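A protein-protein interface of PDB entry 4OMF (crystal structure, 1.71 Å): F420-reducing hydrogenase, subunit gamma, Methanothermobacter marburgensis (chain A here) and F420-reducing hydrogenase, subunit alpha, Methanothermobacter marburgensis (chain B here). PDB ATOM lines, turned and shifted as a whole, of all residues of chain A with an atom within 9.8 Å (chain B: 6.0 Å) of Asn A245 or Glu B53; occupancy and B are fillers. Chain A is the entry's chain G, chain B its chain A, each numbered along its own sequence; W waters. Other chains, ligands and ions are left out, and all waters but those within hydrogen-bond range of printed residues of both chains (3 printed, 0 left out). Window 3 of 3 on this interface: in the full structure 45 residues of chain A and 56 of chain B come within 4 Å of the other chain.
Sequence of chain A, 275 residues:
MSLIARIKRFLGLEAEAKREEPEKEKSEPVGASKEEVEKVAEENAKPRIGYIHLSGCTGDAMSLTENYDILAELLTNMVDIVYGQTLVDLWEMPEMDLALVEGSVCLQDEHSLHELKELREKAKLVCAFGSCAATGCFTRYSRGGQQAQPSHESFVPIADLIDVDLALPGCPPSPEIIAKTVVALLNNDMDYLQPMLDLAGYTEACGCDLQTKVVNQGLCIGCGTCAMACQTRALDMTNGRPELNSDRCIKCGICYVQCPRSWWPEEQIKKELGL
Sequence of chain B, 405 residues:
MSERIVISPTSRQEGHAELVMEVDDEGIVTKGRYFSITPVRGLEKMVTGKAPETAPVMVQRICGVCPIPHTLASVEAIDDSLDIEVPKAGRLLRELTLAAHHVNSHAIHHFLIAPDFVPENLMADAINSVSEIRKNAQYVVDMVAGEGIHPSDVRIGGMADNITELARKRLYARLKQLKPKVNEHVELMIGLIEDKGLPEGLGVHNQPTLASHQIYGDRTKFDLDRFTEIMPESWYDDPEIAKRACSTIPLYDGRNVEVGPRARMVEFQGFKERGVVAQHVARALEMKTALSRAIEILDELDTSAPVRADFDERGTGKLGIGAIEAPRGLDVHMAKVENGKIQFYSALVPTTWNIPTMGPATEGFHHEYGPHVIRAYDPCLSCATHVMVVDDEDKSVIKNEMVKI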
ATOM      1  N   TYR A 141      17.923 -25.197  -1.642  1.00  0.00           N
ATOM      2  CA  TYR A 141      17.455 -25.457  -0.268  1.00  0.00           C
ATOM      3  C   TYR A 141      16.828 -26.846  -0.036  1.00  0.00           C
ATOM      4  O   TYR A 141      16.565 -27.234   1.119  1.00  0.00           O
ATOM      5  CB  TYR A 141      16.428 -24.394   0.163  1.00  0.00           C
ATOM      6  CG  TYR A 141      16.970 -22.994   0.167  1.00  0.00           C
ATOM      7  CD1 TYR A 141      18.031 -22.638   0.989  1.00  0.00           C
ATOM      8  CD2 TYR A 141      16.409 -22.008  -0.639  1.00  0.00           C
ATOM      9  CE1 TYR A 141      18.523 -21.327   1.001  1.00  0.00           C
ATOM     10  CE2 TYR A 141      16.907 -20.706  -0.630  1.00  0.00           C
ATOM     11  CZ  TYR A 141      17.955 -20.383   0.190  1.00  0.00           C
ATOM     12  OH  TYR A 141      18.431 -19.093   0.192  1.00  0.00           O
ATOM     13  N   CYS A 206      24.043 -16.239  -5.098  1.00  0.00           N
ATOM     14  CA  CYS A 206      23.367 -15.845  -3.874  1.00  0.00           C
ATOM     15  C   CYS A 206      23.405 -14.352  -3.714  1.00  0.00           C
ATOM     16  O   CYS A 206      24.239 -13.704  -4.330  1.00  0.00           O
ATOM     17  CB  CYS A 206      24.017 -16.489  -2.668  1.00  0.00           C
ATOM     18  SG  CYS A 206      22.968 -16.148  -1.278  1.00  0.00           S
ATOM     19  N   GLY A 207      22.523 -13.784  -2.896  1.00  0.00           N
ATOM     20  CA  GLY A 207      22.566 -12.348  -2.706  1.00  0.00           C
ATOM     21  C   GLY A 207      23.891 -11.887  -2.098  1.00  0.00           C
ATOM     22  O   GLY A 207      24.262 -10.719  -2.257  1.00  0.00           O
ATOM     23  N   CYS A 208      24.604 -12.788  -1.421  1.00  0.00           N
ATOM     24  CA  CYS A 208      25.905 -12.435  -0.836  1.00  0.00           C
ATOM     25  C   CYS A 208      26.956 -12.184  -1.917  1.00  0.00           C
ATOM     26  O   CYS A 208      28.003 -11.597  -1.628  1.00  0.00           O
ATOM     27  CB  CYS A 208      26.412 -13.549   0.091  1.00  0.00           C
ATOM     28  SG  CYS A 208      25.440 -13.881   1.573  1.00  0.00           S
ATOM     29  N   LEU A 210      26.769  -9.979  -3.957  1.00  0.00           N
ATOM     30  CA  LEU A 210      26.934  -8.526  -4.075  1.00  0.00           C
ATOM     31  C   LEU A 210      28.070  -8.063  -3.163  1.00  0.00           C
ATOM     32  O   LEU A 210      28.802  -7.122  -3.489  1.00  0.00           O
ATOM     33  CB  LEU A 210      25.629  -7.782  -3.733  1.00  0.00           C
ATOM     34  CG  LEU A 210      24.407  -8.123  -4.607  1.00  0.00           C
ATOM     35  CD1 LEU A 210      23.187  -7.345  -4.120  1.00  0.00           C
ATOM     36  CD2 LEU A 210      24.638  -7.860  -6.111  1.00  0.00           C
ATOM     37  N   ALA A 227      18.764  -3.961  -6.042  1.00  0.00           N
ATOM     38  CA  ALA A 227      17.497  -3.952  -5.314  1.00  0.00           C
ATOM     39  C   ALA A 227      16.285  -3.783  -6.257  1.00  0.00           C
ATOM     40  O   ALA A 227      15.220  -4.355  -6.027  1.00  0.00           O
ATOM     41  CB  ALA A 227      17.511  -2.859  -4.254  1.00  0.00           C
ATOM     42  N   CYS A 230      15.741  -7.515  -8.032  1.00  0.00           N
ATOM     43  CA  CYS A 230      15.424  -8.705  -7.228  1.00  0.00           C
ATOM     44  C   CYS A 230      13.939  -9.067  -7.262  1.00  0.00           C
ATOM     45  O   CYS A 230      13.073  -8.295  -6.826  1.00  0.00           O
ATOM     46  CB  CYS A 230      15.851  -8.506  -5.773  1.00  0.00           C
ATOM     47  SG  CYS A 230      15.435  -9.935  -4.758  1.00  0.00           S
ATOM     48  N   THR A 232      12.211 -11.274  -5.669  1.00  0.00           N
ATOM     49  CA  THR A 232      11.548 -11.620  -4.406  1.00  0.00           C
ATOM     50  C   THR A 232      11.497 -10.459  -3.408  1.00  0.00           C
ATOM     51  O   THR A 232      10.934 -10.597  -2.323  1.00  0.00           O
ATOM     52  CB  THR A 232      12.251 -12.792  -3.706  1.00  0.00           C
ATOM     53  OG1 THR A 232      13.582 -12.400  -3.372  1.00  0.00           O
ATOM     54  CG2 THR A 232      12.323 -14.002  -4.651  1.00  0.00           C
ATOM     55  N   ARG A 233      12.089  -9.337  -3.778  1.00  0.00           N
ATOM     56  CA  ARG A 233      12.289  -8.189  -2.878  1.00  0.00           C
ATOM     57  C   ARG A 233      13.124  -8.557  -1.640  1.00  0.00           C
ATOM     58  O   ARG A 233      12.837  -8.086  -0.505  1.00  0.00           O
ATOM     59  CB  ARG A 233      10.939  -7.595  -2.427  1.00  0.00           C
ATOM     60  CG  ARG A 233       9.951  -7.319  -3.556  1.00  0.00           C
ATOM     61  CD  ARG A 233      10.505  -6.360  -4.622  1.00  0.00           C
ATOM     62  NE  ARG A 233       9.432  -6.039  -5.569  1.00  0.00           N
ATOM     63  CZ  ARG A 233       9.149  -6.743  -6.666  1.00  0.00           C
ATOM     64  NH1 ARG A 233       9.872  -7.821  -6.993  1.00  0.00           N
ATOM     65  NH2 ARG A 233       8.124  -6.367  -7.420  1.00  0.00           N
ATOM     66  N   ALA A 234      14.143  -9.393  -1.841  1.00  0.00           N
ATOM     67  CA  ALA A 234      15.062  -9.750  -0.744  1.00  0.00           C
ATOM     68  C   ALA A 234      16.025  -8.614  -0.454  1.00  0.00           C
ATOM     69  O   ALA A 234      16.696  -8.619   0.576  1.00  0.00           O
ATOM     70  CB  ALA A 234      15.861 -11.002  -1.071  1.00  0.00           C
ATOM     71  N   LEU A 235      16.130  -7.663  -1.382  1.00  0.00           N
ATOM     72  CA  LEU A 235      17.105  -6.579  -1.237  1.00  0.00           C
ATOM     73  C   LEU A 235      16.490  -5.223  -0.944  1.00  0.00           C
ATOM     74  O   LEU A 235      15.496  -4.815  -1.561  1.00  0.00           O
ATOM     75  CB  LEU A 235      17.969  -6.452  -2.509  1.00  0.00           C
ATOM     76  CG  LEU A 235      18.935  -7.597  -2.728  1.00  0.00           C
ATOM     77  CD1 LEU A 235      19.557  -7.496  -4.144  1.00  0.00           C
ATOM     78  CD2 LEU A 235      20.035  -7.575  -1.622  1.00  0.00           C
ATOM     79  N   ASP A 236      17.125  -4.521  -0.011  1.00  0.00           N
ATOM     80  CA  ASP A 236      16.854  -3.125   0.261  1.00  0.00           C
ATOM     81  C   ASP A 236      18.197  -2.405   0.120  1.00  0.00           C
ATOM     82  O   ASP A 236      19.186  -3.012  -0.254  1.00  0.00           O
ATOM     83  CB  ASP A 236      16.259  -2.952   1.667  1.00  0.00           C
ATOM     84  CG  ASP A 236      15.483  -1.645   1.841  1.00  0.00           C
ATOM     85  OD1 ASP A 236      15.644  -0.700   1.022  1.00  0.00           O
ATOM     86  OD2 ASP A 236      14.725  -1.574   2.837  1.00  0.00           O
ATOM     87  N   MET A 237      18.225  -1.117   0.420  1.00  0.00           N
ATOM     88  CA  MET A 237      19.488  -0.375   0.478  1.00  0.00           C
ATOM     89  C   MET A 237      19.606   0.285   1.858  1.00  0.00           C
ATOM     90  O   MET A 237      18.645   0.885   2.356  1.00  0.00           O
ATOM     91  CB  MET A 237      19.569   0.694  -0.629  1.00  0.00           C
ATOM     92  CG  MET A 237      19.418   0.149  -2.048  1.00  0.00           C
ATOM     93  SD  MET A 237      20.840  -0.797  -2.612  1.00  0.00           S
ATOM     94  CE  MET A 237      22.098   0.454  -2.823  1.00  0.00           C
ATOM     95  N   THR A 238      20.784   0.157   2.477  1.00  0.00           N
ATOM     96  CA  THR A 238      21.070   0.768   3.770  1.00  0.00           C
ATOM     97  C   THR A 238      22.263   1.674   3.556  1.00  0.00           C
ATOM     98  O   THR A 238      23.315   1.183   3.159  1.00  0.00           O
ATOM     99  CB  THR A 238      21.399  -0.281   4.869  1.00  0.00           C
ATOM    100  OG1 THR A 238      20.259  -1.135   5.085  1.00  0.00           O
ATOM    101  CG2 THR A 238      21.771   0.410   6.201  1.00  0.00           C
ATOM    102  N   ARG A 241      24.056   1.009   0.339  1.00  0.00           N
ATOM    103  CA  ARG A 241      24.670  -0.290   0.111  1.00  0.00           C
ATOM    104  C   ARG A 241      23.601  -1.384   0.194  1.00  0.00           C
ATOM    105  O   ARG A 241      22.622  -1.251   0.926  1.00  0.00           O
ATOM    106  CB  ARG A 241      25.812  -0.547   1.121  1.00  0.00           C
ATOM    107  CG  ARG A 241      27.027   0.367   0.885  1.00  0.00           C
ATOM    108  CD  ARG A 241      27.719   0.038  -0.461  1.00  0.00           C
ATOM    109  NE  ARG A 241      28.951   0.821  -0.687  1.00  0.00           N
ATOM    110  CZ  ARG A 241      29.009   1.974  -1.355  1.00  0.00           C
ATOM    111  NH1 ARG A 241      27.914   2.508  -1.869  1.00  0.00           N
ATOM    112  NH2 ARG A 241      30.176   2.607  -1.519  1.00  0.00           N
ATOM    113  N   PRO A 242      23.752  -2.438  -0.618  1.00  0.00           N
ATOM    114  CA  PRO A 242      22.703  -3.461  -0.629  1.00  0.00           C
ATOM    115  C   PRO A 242      22.528  -4.121   0.717  1.00  0.00           C
ATOM    116  O   PRO A 242      23.525  -4.440   1.394  1.00  0.00           O
ATOM    117  CB  PRO A 242      23.192  -4.468  -1.700  1.00  0.00           C
ATOM    118  CG  PRO A 242      24.655  -4.147  -1.920  1.00  0.00           C
ATOM    119  CD  PRO A 242      24.761  -2.661  -1.669  1.00  0.00           C
ATOM    120  N   GLU A 243      21.267  -4.356   1.093  1.00  0.00           N
ATOM    121  CA  GLU A 243      20.934  -5.008   2.351  1.00  0.00           C
ATOM    122  C   GLU A 243      20.125  -6.277   2.087  1.00  0.00           C
ATOM    123  O   GLU A 243      19.014  -6.203   1.577  1.00  0.00           O
ATOM    124  CB  GLU A 243      20.132  -4.057   3.239  1.00  0.00           C
ATOM    125  CG  GLU A 243      19.999  -4.573   4.668  1.00  0.00           C
ATOM    126  CD  GLU A 243      21.309  -4.448   5.417  1.00  0.00           C
ATOM    127  OE1 GLU A 243      21.681  -3.295   5.715  1.00  0.00           O
ATOM    128  OE2 GLU A 243      21.968  -5.482   5.704  1.00  0.00           O
ATOM    129  N   LEU A 244      20.702  -7.434   2.385  1.00  0.00           N
ATOM    130  CA  LEU A 244      20.063  -8.707   2.008  1.00  0.00           C
ATOM    131  C   LEU A 244      19.155  -9.266   3.110  1.00  0.00           C
ATOM    132  O   LEU A 244      19.587  -9.397   4.255  1.00  0.00           O
ATOM    133  CB  LEU A 244      21.145  -9.737   1.672  1.00  0.00           C
ATOM    134  CG  LEU A 244      20.671 -11.156   1.323  1.00  0.00           C
ATOM    135  CD1 LEU A 244      19.805 -11.128   0.043  1.00  0.00           C
ATOM    136  CD2 LEU A 244      21.865 -12.076   1.131  1.00  0.00           C
ATOM    137  N   ASN A 245      17.899  -9.561   2.762  1.00  0.00           N
ATOM    138  CA  ASN A 245      17.002 -10.297   3.662  1.00  0.00           C
ATOM    139  C   ASN A 245      17.116 -11.747   3.255  1.00  0.00           C
ATOM    140  O   ASN A 245      16.491 -12.177   2.285  1.00  0.00           O
ATOM    141  CB  ASN A 245      15.552  -9.778   3.575  1.00  0.00           C
ATOM    142  CG  ASN A 245      14.569 -10.616   4.399  1.00  0.00           C
ATOM    143  OD1 ASN A 245      14.943 -11.625   5.017  1.00  0.00           O
ATOM    144  ND2 ASN A 245      13.311 -10.178   4.440  1.00  0.00           N
ATOM    145  N   SER A 246      17.955 -12.506   3.962  1.00  0.00           N
ATOM    146  CA  SER A 246      18.241 -13.883   3.561  1.00  0.00           C
ATOM    147  C   SER A 246      17.013 -14.793   3.563  1.00  0.00           C
ATOM    148  O   SER A 246      16.982 -15.810   2.859  1.00  0.00           O
ATOM    149  CB  SER A 246      19.321 -14.483   4.463  1.00  0.00           C
ATOM    150  OG  SER A 246      20.598 -14.120   3.986  1.00  0.00           O
ATOM    151  N   ASP A 247      16.011 -14.426   4.343  1.00  0.00           N
ATOM    152  CA  ASP A 247      14.772 -15.208   4.420  1.00  0.00           C
ATOM    153  C   ASP A 247      14.003 -15.205   3.100  1.00  0.00           C
ATOM    154  O   ASP A 247      13.143 -16.069   2.883  1.00  0.00           O
ATOM    155  CB  ASP A 247      13.856 -14.685   5.521  1.00  0.00           C
ATOM    156  CG  ASP A 247      14.431 -14.899   6.927  1.00  0.00           C
ATOM    157  OD1 ASP A 247      15.358 -15.720   7.093  1.00  0.00           O
ATOM    158  OD2 ASP A 247      13.919 -14.264   7.863  1.00  0.00           O
ATOM    159  N   ARG A 248      14.319 -14.261   2.216  1.00  0.00           N
ATOM    160  CA  ARG A 248      13.617 -14.157   0.924  1.00  0.00           C
ATOM    161  C   ARG A 248      14.505 -14.488  -0.274  1.00  0.00           C
ATOM    162  O   ARG A 248      14.034 -14.451  -1.427  1.00  0.00           O
ATOM    163  CB  ARG A 248      13.022 -12.744   0.732  1.00  0.00           C
ATOM    164  CG  ARG A 248      12.029 -12.299   1.838  1.00  0.00           C
ATOM    165  CD  ARG A 248      11.423 -10.918   1.544  1.00  0.00           C
ATOM    166  NE  ARG A 248      10.539 -11.048   0.389  1.00  0.00           N
ATOM    167  CZ  ARG A 248       9.271 -11.426   0.458  1.00  0.00           C
ATOM    168  NH1 ARG A 248       8.568 -11.571  -0.658  1.00  0.00           N
ATOM    169  NH2 ARG A 248       8.702 -11.672   1.640  1.00  0.00           N
ATOM    170  N   CYS A 249      15.773 -14.826  -0.027  1.00  0.00           N
ATOM    171  CA  CYS A 249      16.703 -15.052  -1.155  1.00  0.00           C
ATOM    172  C   CYS A 249      16.517 -16.437  -1.743  1.00  0.00           C
ATOM    173  O   CYS A 249      16.552 -17.430  -1.001  1.00  0.00           O
ATOM    174  CB  CYS A 249      18.167 -14.885  -0.726  1.00  0.00           C
ATOM    175  SG  CYS A 249      19.315 -14.994  -2.152  1.00  0.00           S
ATOM    176  N   ILE A 250      16.346 -16.502  -3.071  1.00  0.00           N
ATOM    177  CA  ILE A 250      16.137 -17.767  -3.763  1.00  0.00           C
ATOM    178  C   ILE A 250      17.391 -18.195  -4.538  1.00  0.00           C
ATOM    179  O   ILE A 250      17.345 -19.149  -5.313  1.00  0.00           O
ATOM    180  CB  ILE A 250      14.934 -17.670  -4.718  1.00  0.00           C
ATOM    181  CG1 ILE A 250      15.101 -16.443  -5.642  1.00  0.00           C
ATOM    182  CG2 ILE A 250      13.637 -17.534  -3.893  1.00  0.00           C
ATOM    183  CD1 ILE A 250      14.194 -16.455  -6.873  1.00  0.00           C
ATOM    184  N   LYS A 251      18.504 -17.487  -4.335  1.00  0.00           N
ATOM    185  CA  LYS A 251      19.795 -17.898  -4.914  1.00  0.00           C
ATOM    186  C   LYS A 251      19.751 -17.975  -6.447  1.00  0.00           C
ATOM    187  O   LYS A 251      20.368 -18.857  -7.081  1.00  0.00           O
ATOM    188  CB  LYS A 251      20.245 -19.226  -4.309  1.00  0.00           C
ATOM    189  CG  LYS A 251      20.539 -19.095  -2.798  1.00  0.00           C
ATOM    190  CD  LYS A 251      21.029 -20.390  -2.192  1.00  0.00           C
ATOM    191  CE  LYS A 251      21.475 -20.208  -0.743  1.00  0.00           C
ATOM    192  NZ  LYS A 251      22.805 -19.552  -0.698  1.00  0.00           N
ATOM    193  N   ALA B  51      12.088 -19.500   8.922  1.00  0.00           N
ATOM    194  CA  ALA B  51      11.289 -18.346   9.342  1.00  0.00           C
ATOM    195  C   ALA B  51       9.985 -18.312   8.556  1.00  0.00           C
ATOM    196  O   ALA B  51       9.942 -18.678   7.374  1.00  0.00           O
ATOM    197  CB  ALA B  51      12.062 -17.065   9.133  1.00  0.00           C
ATOM    198  N   PRO B  52       8.909 -17.818   9.185  1.00  0.00           N
ATOM    199  CA  PRO B  52       7.636 -17.794   8.454  1.00  0.00           C
ATOM    200  C   PRO B  52       7.678 -17.021   7.119  1.00  0.00           C
ATOM    201  O   PRO B  52       7.003 -17.452   6.167  1.00  0.00           O
ATOM    202  CB  PRO B  52       6.677 -17.120   9.445  1.00  0.00           C
ATOM    203  CG  PRO B  52       7.306 -17.382  10.815  1.00  0.00           C
ATOM    204  CD  PRO B  52       8.775 -17.387  10.592  1.00  0.00           C
ATOM    205  N   GLU B  53       8.458 -15.942   7.038  1.00  0.00           N
ATOM    206  CA  GLU B  53       8.500 -15.119   5.832  1.00  0.00           C
ATOM    207  C   GLU B  53       9.022 -15.933   4.639  1.00  0.00           C
ATOM    208  O   GLU B  53       8.700 -15.649   3.478  1.00  0.00           O
ATOM    209  CB  GLU B  53       9.380 -13.875   6.042  1.00  0.00           C
ATOM    210  CG  GLU B  53       9.474 -13.005   4.798  1.00  0.00           C
ATOM    211  CD  GLU B  53      10.167 -11.679   5.017  1.00  0.00           C
ATOM    212  OE1 GLU B  53      11.013 -11.566   5.936  1.00  0.00           O
ATOM    213  OE2 GLU B  53       9.832 -10.735   4.262  1.00  0.00           O
ATOM    214  N   THR B  54       9.813 -16.955   4.940  1.00  0.00           N
ATOM    215  CA  THR B  54      10.417 -17.770   3.890  1.00  0.00           C
ATOM    216  C   THR B  54       9.384 -18.659   3.203  1.00  0.00           C
ATOM    217  O   THR B  54       9.475 -18.932   1.996  1.00  0.00           O
ATOM    218  CB  THR B  54      11.563 -18.637   4.460  1.00  0.00           C
ATOM    219  OG1 THR B  54      12.625 -17.777   4.904  1.00  0.00           O
ATOM    220  CG2 THR B  54      12.105 -19.607   3.413  1.00  0.00           C
ATOM    221  N   ALA B  55       8.372 -19.104   3.942  1.00  0.00           N
ATOM    222  CA  ALA B  55       7.490 -20.095   3.358  1.00  0.00           C
ATOM    223  C   ALA B  55       6.724 -19.611   2.090  1.00  0.00           C
ATOM    224  O   ALA B  55       6.716 -20.317   1.095  1.00  0.00           O
ATOM    225  CB  ALA B  55       6.539 -20.623   4.427  1.00  0.00           C
ATOM    226  N   PRO B  56       6.087 -18.416   2.109  1.00  0.00           N
ATOM    227  CA  PRO B  56       5.389 -17.992   0.873  1.00  0.00           C
ATOM    228  C   PRO B  56       6.302 -17.823  -0.345  1.00  0.00           C
ATOM    229  O   PRO B  56       5.901 -18.101  -1.475  1.00  0.00           O
ATOM    230  CB  PRO B  56       4.780 -16.636   1.255  1.00  0.00           C
ATOM    231  CG  PRO B  56       4.617 -16.710   2.760  1.00  0.00           C
ATOM    232  CD  PRO B  56       5.832 -17.495   3.232  1.00  0.00           C
ATOM    233  N   VAL B  57       7.519 -17.347  -0.116  1.00  0.00           N
ATOM    234  CA  VAL B  57       8.510 -17.206  -1.186  1.00  0.00           C
ATOM    235  C   VAL B  57       8.875 -18.554  -1.807  1.00  0.00           C
ATOM    236  O   VAL B  57       8.940 -18.685  -3.032  1.00  0.00           O
ATOM    237  CB  VAL B  57       9.780 -16.526  -0.657  1.00  0.00           C
ATOM    238  CG1 VAL B  57      10.872 -16.463  -1.742  1.00  0.00           C
ATOM    239  CG2 VAL B  57       9.420 -15.093  -0.099  1.00  0.00           C
ATOM    240  N   MET B  58       9.137 -19.550  -0.963  1.00  0.00           N
ATOM    241  CA  MET B  58       9.495 -20.858  -1.481  1.00  0.00           C
ATOM    242  C   MET B  58       8.290 -21.640  -2.033  1.00  0.00           C
ATOM    243  O   MET B  58       8.368 -22.225  -3.127  1.00  0.00           O
ATOM    244  CB  MET B  58      10.206 -21.681  -0.407  1.00  0.00           C
ATOM    245  CG  MET B  58      11.429 -20.993   0.190  1.00  0.00           C
ATOM    246  SD  MET B  58      12.623 -20.546  -1.117  1.00  0.00           S
ATOM    247  CE  MET B  58      13.487 -19.155  -0.368  1.00  0.00           C
ATOM    248  N   ILE B  78      -0.463 -19.075   7.610  1.00  0.00           N
ATOM    249  CA  ILE B  78       0.409 -18.480   8.611  1.00  0.00           C
ATOM    250  C   ILE B  78      -0.364 -17.397   9.404  1.00  0.00           C
ATOM    251  O   ILE B  78      -0.248 -17.327  10.628  1.00  0.00           O
ATOM    252  CB  ILE B  78       1.707 -17.918   7.953  1.00  0.00           C
ATOM    253  CG1 ILE B  78       2.587 -19.074   7.491  1.00  0.00           C
ATOM    254  CG2 ILE B  78       2.484 -17.023   8.947  1.00  0.00           C
ATOM    255  CD1 ILE B  78       3.626 -18.696   6.395  1.00  0.00           C
ATOM    256  N   ARG B 155       1.741 -11.000   1.337  1.00  0.00           N
ATOM    257  CA  ARG B 155       2.586 -11.072   2.550  1.00  0.00           C
ATOM    258  C   ARG B 155       1.785 -11.567   3.746  1.00  0.00           C
ATOM    259  O   ARG B 155       0.556 -11.465   3.769  1.00  0.00           O
ATOM    260  CB  ARG B 155       3.168  -9.681   2.900  1.00  0.00           C
ATOM    261  CG  ARG B 155       4.038  -9.051   1.821  1.00  0.00           C
ATOM    262  CD  ARG B 155       5.350  -9.814   1.616  1.00  0.00           C
ATOM    263  NE  ARG B 155       6.072  -9.152   0.534  1.00  0.00           N
ATOM    264  CZ  ARG B 155       6.921  -8.143   0.700  1.00  0.00           C
ATOM    265  NH1 ARG B 155       7.225  -7.706   1.921  1.00  0.00           N
ATOM    266  NH2 ARG B 155       7.493  -7.583  -0.356  1.00  0.00           N
ATOM    267  N   ILE B 156       2.479 -12.132   4.734  1.00  0.00           N
ATOM    268  CA  ILE B 156       1.869 -12.390   6.030  1.00  0.00           C
ATOM    269  C   ILE B 156       1.284 -11.080   6.529  1.00  0.00           C
ATOM    270  O   ILE B 156       1.946 -10.051   6.494  1.00  0.00           O
ATOM    271  CB  ILE B 156       2.896 -12.948   7.046  1.00  0.00           C
ATOM    272  CG1 ILE B 156       3.475 -14.264   6.520  1.00  0.00           C
ATOM    273  CG2 ILE B 156       2.259 -13.104   8.478  1.00  0.00           C
ATOM    274  CD1 ILE B 156       4.681 -14.762   7.303  1.00  0.00           C
ATOM    275  N   ARG B 308      -2.000  -4.026   5.483  1.00  0.00           N
ATOM    276  CA  ARG B 308      -1.223  -5.014   6.213  1.00  0.00           C
ATOM    277  C   ARG B 308      -1.317  -4.781   7.714  1.00  0.00           C
ATOM    278  O   ARG B 308      -1.186  -3.651   8.184  1.00  0.00           O
ATOM    279  CB  ARG B 308       0.230  -4.976   5.765  1.00  0.00           C
ATOM    280  CG  ARG B 308       0.979  -6.265   6.113  1.00  0.00           C
ATOM    281  CD  ARG B 308       2.439  -6.198   5.692  1.00  0.00           C
ATOM    282  NE  ARG B 308       3.080  -7.472   5.974  1.00  0.00           N
ATOM    283  CZ  ARG B 308       4.359  -7.731   5.733  1.00  0.00           C
ATOM    284  NH1 ARG B 308       5.141  -6.794   5.211  1.00  0.00           N
ATOM    285  NH2 ARG B 308       4.863  -8.924   6.031  1.00  0.00           N
ATOM    286  N   GLU B 313       5.581 -12.501  15.195  1.00  0.00           N
ATOM    287  CA  GLU B 313       5.771 -13.729  14.426  1.00  0.00           C
ATOM    288  C   GLU B 313       6.232 -14.942  15.250  1.00  0.00           C
ATOM    289  O   GLU B 313       6.513 -16.005  14.686  1.00  0.00           O
ATOM    290  CB  GLU B 313       6.772 -13.475  13.285  1.00  0.00           C
ATOM    291  CG  GLU B 313       8.231 -13.446  13.716  1.00  0.00           C
ATOM    292  CD  GLU B 313       9.188 -13.088  12.572  1.00  0.00           C
ATOM    293  OE1 GLU B 313       9.125 -11.931  12.091  1.00  0.00           O
ATOM    294  OE2 GLU B 313       9.997 -13.957  12.161  1.00  0.00           O
HETATM  295  O   HOH W   1      11.879 -12.797   8.244  1.00  0.00           O
HETATM  296  O   HOH W   2      10.595  -7.109   0.996  1.00  0.00           O
HETATM  297  O   HOH W   3       6.835 -14.014   2.467  1.00  0.00           O
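ND2 of Asn A245 sits at hydrogen-bond distance from OE1 of Glu B53 (3.1 Å).
The side-chain hydroxyl (OG1) of Thr B54 lies within hydrogen-bond range of the backbone carbonyl oxygen (O) of Asp A247, 2.7 Å away.
OE2 of Glu B53 is in salt-bridge range of NH2 of Arg A248 (3.0 Å).
O of Thr A232 is in hydrogen-bond range of NE of Arg A248.
The side-chain amide oxygen of Asn A245 sits at hydrogen-bond distance from the backbone NH of Asp A247 (3.1 Å).
OH of Tyr A141 sits at hydrogen-bond distance from O of Cys A249, at 2.8 Å.
N of Lys A251 sits close to SG of Cys A249, at 3.4 Å.
SG of Cys A249 sits close to N of Gly A207 (3.5 Å).
Among the printed residues, merely in contact across the chains: Cys A249 with Met B58 (3.6 Å), Asp A247 with Ala B51 (3.6 Å), Ile A250 with Val B57 (3.7 Å), Arg A248 with Val B57 (3.7 Å), Arg A248 with Arg B155 (3.7 Å), Tyr A141 with Met B58 (3.8 Å) and Ile A250 with Met B58 (3.9 Å).
Asn A245 touches just one residue of chain B: Glu B53.
Printed residues of chain B within 4 Å of Arg A248: Glu B53 (3.0 Å), Val B57 (3.7 Å) and Arg B155 (3.7 Å).
Of chain A, only Asp A247 comes within 4 Å of Ala B51.
No residue of chain A comes within 4 Å of Pro B52.
Of chain A, only Asn A245 (3.1 Å) and Arg A248 (3.0 Å) come within 4 Å of Glu B53.
Of chain A, only Asp A247 comes within 4 Å of Thr B54.
No residue of chain A comes within 4 Å of Ala B55.
Of the printed residues of chain A, Met B58 touches Tyr A141 (3.8 Å), Cys A249 (3.6 Å) and Ile A250 (3.9 Å).
Of the printed residues of chain A, Arg B155 touches Arg A248.
The nearest residue of chain A that does not touch Glu B53 is Asp A247 (4.2 Å).
The nearest printed residue of chain B that does not touch Cys A249 is Val B57 (5.4 Å).
Of the 25 printed residues of chain A, 6 touch a printed residue of chain B.
Hydrophobic or aromatic side chains of chain A that line the printed part of chain B: Tyr A141 and Ile A250.
Hydrophobic or aromatic side chains of chain B within 4 Å of the printed part of chain A: Ala B51, Val B57 and Met B58.
Among the printed residues, 10 pairs touch across the chains.
Water W1 bridges the side-chain carboxylate (OD2) of Asp A247 (2.5 Å) and the side-chain carboxylate (OE1) of Glu B53 (2.8 Å).
Water W3 bridges the backbone carbonyl oxygen of Glu B53 (2.7 Å) and the guanidinium group of Arg A248 (3.1 Å).
Water W2 lies within hydrogen-bond range of the backbone carbonyl oxygen (O) of Arg A233 and the guanidinium group (NH2) of Arg B155.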
